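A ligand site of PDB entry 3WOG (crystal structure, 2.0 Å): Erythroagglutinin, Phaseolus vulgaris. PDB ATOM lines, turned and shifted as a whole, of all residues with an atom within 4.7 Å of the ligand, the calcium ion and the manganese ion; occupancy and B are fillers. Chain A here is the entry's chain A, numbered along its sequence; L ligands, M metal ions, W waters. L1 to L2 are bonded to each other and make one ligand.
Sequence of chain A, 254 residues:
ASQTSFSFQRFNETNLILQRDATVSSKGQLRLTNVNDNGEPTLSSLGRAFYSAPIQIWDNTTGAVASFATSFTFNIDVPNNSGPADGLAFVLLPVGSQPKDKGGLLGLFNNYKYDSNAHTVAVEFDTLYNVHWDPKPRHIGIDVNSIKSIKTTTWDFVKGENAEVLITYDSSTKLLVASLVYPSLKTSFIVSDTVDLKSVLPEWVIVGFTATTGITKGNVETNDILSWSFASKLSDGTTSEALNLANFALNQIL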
ATOM      1  N   ASP A  86      22.200   9.513   6.784  1.00  0.00           N
ATOM      2  CA  ASP A  86      22.053  10.618   7.755  1.00  0.00           C
ATOM      3  C   ASP A  86      23.385  11.217   8.213  1.00  0.00           C
ATOM      4  O   ASP A  86      23.456  12.355   8.667  1.00  0.00           O
ATOM      5  CB  ASP A  86      21.301  10.122   8.972  1.00  0.00           C
ATOM      6  CG  ASP A  86      19.827  10.347   8.852  1.00  0.00           C
ATOM      7  OD1 ASP A  86      19.402  11.526   8.945  1.00  0.00           O
ATOM      8  OD2 ASP A  86      19.103   9.338   8.646  1.00  0.00           O
ATOM      9  N   LYS A 102      18.069   4.625  15.046  1.00  0.00           N
ATOM     10  CA  LYS A 102      18.678   4.831  13.739  1.00  0.00           C
ATOM     11  C   LYS A 102      18.359   6.233  13.146  1.00  0.00           C
ATOM     12  O   LYS A 102      17.949   7.146  13.879  1.00  0.00           O
ATOM     13  CB  LYS A 102      18.248   3.706  12.798  1.00  0.00           C
ATOM     14  CG  LYS A 102      16.736   3.580  12.659  1.00  0.00           C
ATOM     15  CD  LYS A 102      16.363   2.583  11.566  1.00  0.00           C
ATOM     16  CE  LYS A 102      16.551   1.139  12.016  1.00  0.00           C
ATOM     17  NZ  LYS A 102      16.420   0.167  10.887  1.00  0.00           N
ATOM     18  N   GLY A 103      18.579   6.416  11.845  1.00  0.00           N
ATOM     19  CA  GLY A 103      18.281   7.694  11.192  1.00  0.00           C
ATOM     20  C   GLY A 103      19.037   8.866  11.776  1.00  0.00           C
ATOM     21  O   GLY A 103      20.236   8.773  12.048  1.00  0.00           O
ATOM     22  N   GLY A 104      18.345   9.985  11.982  1.00  0.00           N
ATOM     23  CA  GLY A 104      18.993  11.205  12.454  1.00  0.00           C
ATOM     24  C   GLY A 104      19.561  11.151  13.866  1.00  0.00           C
ATOM     25  O   GLY A 104      20.267  12.055  14.282  1.00  0.00           O
ATOM     26  N   LEU A 105      19.236  10.118  14.628  1.00  0.00           N
ATOM     27  CA  LEU A 105      19.815   9.946  15.963  1.00  0.00           C
ATOM     28  C   LEU A 105      21.173   9.224  15.934  1.00  0.00           C
ATOM     29  O   LEU A 105      21.827   9.033  16.975  1.00  0.00           O
ATOM     30  CB  LEU A 105      18.796   9.237  16.873  1.00  0.00           C
ATOM     31  CG  LEU A 105      17.503  10.050  17.056  1.00  0.00           C
ATOM     32  CD1 LEU A 105      16.427   9.285  17.846  1.00  0.00           C
ATOM     33  CD2 LEU A 105      17.774  11.389  17.706  1.00  0.00           C
ATOM     34  N   TYR A 112      15.658  13.406  21.025  1.00  0.00           N
ATOM     35  CA  TYR A 112      16.496  14.578  20.881  1.00  0.00           C
ATOM     36  C   TYR A 112      16.657  15.471  22.098  1.00  0.00           C
ATOM     37  O   TYR A 112      17.132  16.600  21.986  1.00  0.00           O
ATOM     38  CB  TYR A 112      16.150  15.406  19.640  1.00  0.00           C
ATOM     39  CG  TYR A 112      14.703  15.811  19.458  1.00  0.00           C
ATOM     40  CD1 TYR A 112      14.256  17.094  19.816  1.00  0.00           C
ATOM     41  CD2 TYR A 112      13.779  14.935  18.869  1.00  0.00           C
ATOM     42  CE1 TYR A 112      12.934  17.477  19.619  1.00  0.00           C
ATOM     43  CE2 TYR A 112      12.461  15.306  18.653  1.00  0.00           C
ATOM     44  CZ  TYR A 112      12.044  16.564  19.032  1.00  0.00           C
ATOM     45  OH  TYR A 112      10.728  16.914  18.807  1.00  0.00           O
ATOM     46  N   GLU A 124      30.156  14.683  14.943  1.00  0.00           N
ATOM     47  CA  GLU A 124      29.274  14.239  13.875  1.00  0.00           C
ATOM     48  C   GLU A 124      29.551  14.940  12.557  1.00  0.00           C
ATOM     49  O   GLU A 124      29.940  16.114  12.518  1.00  0.00           O
ATOM     50  CB  GLU A 124      27.786  14.474  14.256  1.00  0.00           C
ATOM     51  CG  GLU A 124      27.358  15.920  14.476  1.00  0.00           C
ATOM     52  CD  GLU A 124      25.838  16.074  14.573  1.00  0.00           C
ATOM     53  OE1 GLU A 124      25.217  15.256  15.309  1.00  0.00           O
ATOM     54  OE2 GLU A 124      25.245  16.957  13.876  1.00  0.00           O
ATOM     55  N   ASP A 126      27.152  15.485   9.696  1.00  0.00           N
ATOM     56  CA  ASP A 126      25.682  15.340   9.598  1.00  0.00           C
ATOM     57  C   ASP A 126      25.269  15.817   8.207  1.00  0.00           C
ATOM     58  O   ASP A 126      25.470  16.981   7.849  1.00  0.00           O
ATOM     59  CB  ASP A 126      25.017  16.204  10.729  1.00  0.00           C
ATOM     60  CG  ASP A 126      23.507  15.985  10.855  1.00  0.00           C
ATOM     61  OD1 ASP A 126      22.930  15.452   9.893  1.00  0.00           O
ATOM     62  OD2 ASP A 126      22.901  16.374  11.932  1.00  0.00           O
ATOM     63  N   LEU A 128      22.118  15.486   6.845  1.00  0.00           N
ATOM     64  CA  LEU A 128      20.685  15.708   6.673  1.00  0.00           C
ATOM     65  C   LEU A 128      20.109  16.572   7.784  1.00  0.00           C
ATOM     66  O   LEU A 128      20.226  16.249   8.975  1.00  0.00           O
ATOM     67  CB  LEU A 128      19.950  14.369   6.588  1.00  0.00           C
ATOM     68  CG  LEU A 128      18.436  14.568   6.360  1.00  0.00           C
ATOM     69  CD1 LEU A 128      17.961  13.836   5.120  1.00  0.00           C
ATOM     70  CD2 LEU A 128      17.577  14.291   7.591  1.00  0.00           C
ATOM     71  N   TYR A 129      19.497  17.684   7.360  1.00  0.00           N
ATOM     72  CA  TYR A 129      18.799  18.605   8.247  1.00  0.00           C
ATOM     73  C   TYR A 129      17.597  17.968   8.953  1.00  0.00           C
ATOM     74  O   TYR A 129      16.619  17.558   8.324  1.00  0.00           O
ATOM     75  CB  TYR A 129      18.357  19.838   7.445  1.00  0.00           C
ATOM     76  CG  TYR A 129      17.359  20.785   8.111  1.00  0.00           C
ATOM     77  CD1 TYR A 129      17.708  21.501   9.253  1.00  0.00           C
ATOM     78  CD2 TYR A 129      16.099  20.997   7.548  1.00  0.00           C
ATOM     79  CE1 TYR A 129      16.812  22.399   9.846  1.00  0.00           C
ATOM     80  CE2 TYR A 129      15.187  21.874   8.119  1.00  0.00           C
ATOM     81  CZ  TYR A 129      15.545  22.580   9.263  1.00  0.00           C
ATOM     82  OH  TYR A 129      14.657  23.457   9.819  1.00  0.00           O
ATOM     83  N   ASN A 130      17.676  17.889  10.273  1.00  0.00           N
ATOM     84  CA  ASN A 130      16.582  17.379  11.069  1.00  0.00           C
ATOM     85  C   ASN A 130      15.937  18.569  11.747  1.00  0.00           C
ATOM     86  O   ASN A 130      16.552  19.201  12.633  1.00  0.00           O
ATOM     87  CB  ASN A 130      17.093  16.368  12.097  1.00  0.00           C
ATOM     88  CG  ASN A 130      17.493  15.054  11.469  1.00  0.00           C
ATOM     89  OD1 ASN A 130      18.693  14.776  11.272  1.00  0.00           O
ATOM     90  ND2 ASN A 130      16.503  14.232  11.119  1.00  0.00           N
ATOM     91  N   VAL A 131      14.718  18.900  11.301  1.00  0.00           N
ATOM     92  CA  VAL A 131      14.053  20.158  11.679  1.00  0.00           C
ATOM     93  C   VAL A 131      14.005  20.462  13.187  1.00  0.00           C
ATOM     94  O   VAL A 131      14.082  21.628  13.610  1.00  0.00           O
ATOM     95  CB  VAL A 131      12.613  20.217  11.075  1.00  0.00           C
ATOM     96  CG1 VAL A 131      11.727  19.110  11.638  1.00  0.00           C
ATOM     97  CG2 VAL A 131      11.989  21.576  11.302  1.00  0.00           C
ATOM     98  N   HIS A 132      13.864  19.432  14.019  1.00  0.00           N
ATOM     99  CA  HIS A 132      13.694  19.660  15.453  1.00  0.00           C
ATOM    100  C   HIS A 132      14.979  19.991  16.178  1.00  0.00           C
ATOM    101  O   HIS A 132      14.936  20.367  17.347  1.00  0.00           O
ATOM    102  CB  HIS A 132      13.006  18.494  16.127  1.00  0.00           C
ATOM    103  CG  HIS A 132      11.590  18.254  15.633  1.00  0.00           C
ATOM    104  ND1 HIS A 132      10.672  19.240  15.537  1.00  0.00           N
ATOM    105  CD2 HIS A 132      10.951  17.081  15.235  1.00  0.00           C
ATOM    106  CE1 HIS A 132       9.506  18.732  15.080  1.00  0.00           C
ATOM    107  NE2 HIS A 132       9.681  17.398  14.892  1.00  0.00           N
ATOM    108  N   TRP A 133      16.144  19.866  15.523  1.00  0.00           N
ATOM    109  CA  TRP A 133      17.385  20.214  16.246  1.00  0.00           C
ATOM    110  C   TRP A 133      18.561  20.693  15.447  1.00  0.00           C
ATOM    111  O   TRP A 133      19.450  21.321  16.017  1.00  0.00           O
ATOM    112  CB  TRP A 133      17.833  19.069  17.139  1.00  0.00           C
ATOM    113  CG  TRP A 133      18.250  17.850  16.350  1.00  0.00           C
ATOM    114  CD1 TRP A 133      19.464  17.625  15.700  1.00  0.00           C
ATOM    115  CD2 TRP A 133      17.447  16.663  16.090  1.00  0.00           C
ATOM    116  NE1 TRP A 133      19.464  16.394  15.077  1.00  0.00           N
ATOM    117  CE2 TRP A 133      18.285  15.763  15.271  1.00  0.00           C
ATOM    118  CE3 TRP A 133      16.163  16.239  16.442  1.00  0.00           C
ATOM    119  CZ2 TRP A 133      17.827  14.529  14.844  1.00  0.00           C
ATOM    120  CZ3 TRP A 133      15.724  14.980  16.007  1.00  0.00           C
ATOM    121  CH2 TRP A 133      16.541  14.154  15.241  1.00  0.00           C
ATOM    122  N   ASP A 134      18.629  20.380  14.148  1.00  0.00           N
ATOM    123  CA  ASP A 134      19.831  20.705  13.349  1.00  0.00           C
ATOM    124  C   ASP A 134      19.854  22.136  12.832  1.00  0.00           C
ATOM    125  O   ASP A 134      18.787  22.718  12.569  1.00  0.00           O
ATOM    126  CB  ASP A 134      19.925  19.788  12.133  1.00  0.00           C
ATOM    127  CG  ASP A 134      20.608  18.446  12.437  1.00  0.00           C
ATOM    128  OD1 ASP A 134      21.582  18.342  13.264  1.00  0.00           O
ATOM    129  OD2 ASP A 134      20.156  17.480  11.782  1.00  0.00           O
ATOM    130  N   HIS A 139      26.734  20.055   8.251  1.00  0.00           N
ATOM    131  CA  HIS A 139      27.524  20.599   9.354  1.00  0.00           C
ATOM    132  C   HIS A 139      28.426  19.586  10.013  1.00  0.00           C
ATOM    133  O   HIS A 139      28.140  18.397   9.992  1.00  0.00           O
ATOM    134  CB  HIS A 139      26.592  21.255  10.406  1.00  0.00           C
ATOM    135  CG  HIS A 139      25.501  20.328  10.957  1.00  0.00           C
ATOM    136  ND1 HIS A 139      24.323  20.149  10.343  1.00  0.00           N
ATOM    137  CD2 HIS A 139      25.450  19.573  12.145  1.00  0.00           C
ATOM    138  CE1 HIS A 139      23.555  19.303  11.052  1.00  0.00           C
ATOM    139  NE2 HIS A 139      24.243  18.944  12.170  1.00  0.00           N
ATOM    140  N   ILE A 147      21.887  14.699  20.631  1.00  0.00           N
ATOM    141  CA  ILE A 147      21.949  14.848  19.171  1.00  0.00           C
ATOM    142  C   ILE A 147      21.964  16.333  18.779  1.00  0.00           C
ATOM    143  O   ILE A 147      22.334  16.702  17.651  1.00  0.00           O
ATOM    144  CB  ILE A 147      20.789  14.077  18.475  1.00  0.00           C
ATOM    145  CG1 ILE A 147      21.108  13.745  17.005  1.00  0.00           C
ATOM    146  CG2 ILE A 147      19.469  14.846  18.584  1.00  0.00           C
ATOM    147  CD1 ILE A 147      22.416  12.997  16.787  1.00  0.00           C
ATOM    148  N   SER A 149      23.834  19.358  18.793  1.00  0.00           N
ATOM    149  CA  SER A 149      25.248  19.692  18.986  1.00  0.00           C
ATOM    150  C   SER A 149      25.443  20.930  19.847  1.00  0.00           C
ATOM    151  O   SER A 149      24.689  21.909  19.729  1.00  0.00           O
ATOM    152  CB  SER A 149      25.959  19.879  17.642  1.00  0.00           C
ATOM    153  OG  SER A 149      25.672  18.789  16.771  1.00  0.00           O
ATOM    154  N   GLY A 214      19.377   7.136   5.631  1.00  0.00           N
ATOM    155  CA  GLY A 214      18.023   7.688   5.806  1.00  0.00           C
ATOM    156  C   GLY A 214      16.983   6.594   5.923  1.00  0.00           C
ATOM    157  O   GLY A 214      17.160   5.484   5.417  1.00  0.00           O
ATOM    158  N   ILE A 215      15.896   6.893   6.618  1.00  0.00           N
ATOM    159  CA  ILE A 215      14.795   5.958   6.684  1.00  0.00           C
ATOM    160  C   ILE A 215      13.833   6.132   5.487  1.00  0.00           C
ATOM    161  O   ILE A 215      13.135   5.187   5.113  1.00  0.00           O
ATOM    162  CB  ILE A 215      14.069   5.953   8.055  1.00  0.00           C
ATOM    163  CG1 ILE A 215      13.272   7.245   8.282  1.00  0.00           C
ATOM    164  CG2 ILE A 215      15.062   5.725   9.199  1.00  0.00           C
ATOM    165  CD1 ILE A 215      12.167   7.081   9.315  1.00  0.00           C
ATOM    166  N   THR A 216      13.815   7.312   4.878  1.00  0.00           N
ATOM    167  CA  THR A 216      12.874   7.650   3.816  1.00  0.00           C
ATOM    168  C   THR A 216      13.528   7.565   2.446  1.00  0.00           C
ATOM    169  O   THR A 216      14.571   8.166   2.217  1.00  0.00           O
ATOM    170  CB  THR A 216      12.279   9.061   4.018  1.00  0.00           C
ATOM    171  OG1 THR A 216      11.629   9.108   5.296  1.00  0.00           O
ATOM    172  CG2 THR A 216      11.243   9.397   2.955  1.00  0.00           C
ATOM    173  N   ASN A 219      16.799   9.403   0.492  1.00  0.00           N
ATOM    174  CA  ASN A 219      17.757   9.953   1.450  1.00  0.00           C
ATOM    175  C   ASN A 219      18.685   8.830   1.926  1.00  0.00           C
ATOM    176  O   ASN A 219      18.302   8.028   2.763  1.00  0.00           O
ATOM    177  CB  ASN A 219      17.013  10.584   2.632  1.00  0.00           C
ATOM    178  CG  ASN A 219      16.033  11.656   2.196  1.00  0.00           C
ATOM    179  OD1 ASN A 219      16.407  12.809   2.009  1.00  0.00           O
ATOM    180  ND2 ASN A 219      14.768  11.279   2.053  1.00  0.00           N
HETATM  181  C1  LIG L   1      12.043  10.974  11.515  1.00  0.00           C
HETATM  182  C2  LIG L   1      13.356  10.739  10.760  1.00  0.00           C
HETATM  183  C3  LIG L   1      14.410  10.149  11.691  1.00  0.00           C
HETATM  184  C4  LIG L   1      14.626  11.106  12.871  1.00  0.00           C
HETATM  185  C5  LIG L   1      13.285  11.348  13.560  1.00  0.00           C
HETATM  186  C6  LIG L   1      13.357  12.406  14.659  1.00  0.00           C
HETATM  187  O1  LIG L   1      11.441   9.760  11.940  1.00  0.00           O
HETATM  188  O2  LIG L   1      13.858  11.980  10.310  1.00  0.00           O
HETATM  189  O3  LIG L   1      15.620   9.980  10.966  1.00  0.00           O
HETATM  190  O4  LIG L   1      15.603  10.621  13.768  1.00  0.00           O
HETATM  191  O5  LIG L   1      12.297  11.804  12.635  1.00  0.00           O
HETATM  192  O6  LIG L   1      12.333  12.116  15.592  1.00  0.00           O
HETATM  193  C1  LG2 L   2      13.437  12.283   8.972  1.00  0.00           C
HETATM  194  C2  LG2 L   2      13.248  13.793   8.871  1.00  0.00           C
HETATM  195  C3  LG2 L   2      12.898  14.259   7.436  1.00  0.00           C
HETATM  196  C4  LG2 L   2      13.829  13.598   6.407  1.00  0.00           C
HETATM  197  C5  LG2 L   2      13.949  12.077   6.648  1.00  0.00           C
HETATM  198  C6  LG2 L   2      14.968  11.416   5.725  1.00  0.00           C
HETATM  199  C7  LG2 L   2      12.487  14.849  10.925  1.00  0.00           C
HETATM  200  C8  LG2 L   2      11.275  15.154  11.765  1.00  0.00           C
HETATM  201  N1  LG2 L   2      12.223  14.170   9.805  1.00  0.00           N
HETATM  202  O1  LG2 L   2      12.984  15.671   7.320  1.00  0.00           O
HETATM  203  O2  LG2 L   2      13.383  13.923   5.093  1.00  0.00           O
HETATM  204  O3  LG2 L   2      14.334  11.802   7.995  1.00  0.00           O
HETATM  205  O4  LG2 L   2      14.971  10.011   5.923  1.00  0.00           O
HETATM  206  O5  LG2 L   2      13.622  15.238  11.257  1.00  0.00           O
HETATM  207 CA    CA M   1      20.911  15.408  11.066  1.00  0.00          CA
HETATM  208 MN    MN M   2      23.434  17.614  13.387  1.00  0.00          MN
HETATM  209  O   HOH W   1      21.051  13.293  10.108  1.00  0.00           O
HETATM  210  O   HOH W   2      23.756  18.861  14.845  1.00  0.00           O
HETATM  211  O   HOH W   3      13.939  16.581  13.654  1.00  0.00           O
HETATM  212  O   HOH W   4      22.820  16.379  14.750  1.00  0.00           O
HETATM  213  O   HOH W   5      21.118  14.599  13.254  1.00  0.00           O
HETATM  214  O   HOH W   6      16.920  11.844   9.629  1.00  0.00           O
HETATM  215  O   HOH W   7      13.846  17.718   8.775  1.00  0.00           O
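Within 4 Å of the manganese ion: Glu 124, Asp 126, Asp 134 and His 139.
The nearest printed residue that does not touch the manganese ion is Ser 149 (4.2 Å).
An oxygen (O5) of LG2 L2 is in hydrogen-bond range of the side-chain amide nitrogen (ND2) of Asn 130 (3.1 Å).
The backbone NH of Gly 104 sits at hydrogen-bond distance from an oxygen (O3) of LIG L1 (2.9 Å).
An oxygen (O4) of LG2 L2 is in hydrogen-bond range of the backbone NH (N) of Thr 216 (3.1 Å).
N of Ile 215 sits at hydrogen-bond distance from O4 of LG2 L2, 3.3 Å away.
Water W5 bridges the backbone carbonyl oxygen (O) of Gly 104 and the indole nitrogen (NE1) of Trp 133.
Water W4 lies within hydrogen-bond range of the side-chain carboxylate of Glu 124 (2.7 Å), the backbone carbonyl oxygen of Ile 147 (3.0 Å) and the indole nitrogen of Trp 133 (3.4 Å).
Water W6 lies within hydrogen-bond range of OD1 of Asp 86 (2.6 Å), O3 of LIG L1 (2.6 Å), ND2 of Asn 130 (2.8 Å) and N of Gly 104 (3.3 Å).
Water W7 lies within hydrogen-bond range of O1 of LG2 L2 (2.7 Å), O of Tyr 129 (2.8 Å) and N of Val 131 (2.9 Å).
Water W3 lies within hydrogen-bond range of an oxygen (O5) of LG2 L2, the backbone NH (N) of His 132 and the backbone NH (N) of Val 131.
The side-chain hydroxyl (OG) of Ser 149 lies close to the side-chain carboxylate (OE2) of Glu 124 (3.5 Å).
The side-chain carboxylate of Asp 134 sits close to the indole nitrogen of Trp 133 (3.4 Å).
OD2 of Asp 86 is in hydrogen-bond range of N of Gly 104 (3.5 Å).
The backbone carbonyl oxygen of Thr 216 sits at hydrogen-bond distance from the side-chain amide nitrogen of Asn 219, 3.1 Å away.
The backbone carbonyl oxygen (O) of Asn 219 lies close to the backbone NH (N) of Gly 214 (3.2 Å).
The manganese ion is bound by water W4, water W2, NE2 of His 139, OD2 of Asp 126, OE2 of Glu 124 and OD1 of Asp 134.
Gly 103 touches the ligand.
Leu 105 touches the ligand.
N of Val 131 touches O5 of LG2 L2, at 3.8 Å.
His 132 touches the ligand.
Trp 133 touches the ligand.
CA of Gly 214 touches O4 of LG2 L2, at 3.8 Å.
ND2 of Asn 219 touches C6 of LG2 L2 (3.7 Å).
Of the 22 residues printed, 12 come within 4 Å of the ligand.
The calcium ion is bound by OD1 of Asn 130 (2.3 Å), OD2 of Asp 134 (2.3 Å), water W1 (2.3 Å), OD1 of Asp 126 (2.3 Å), water W5 (2.3 Å), O of Leu 128 (2.4 Å) and OD2 of Asp 126 (2.4 Å).
The calcium ion has seven donor atoms within binding distance.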
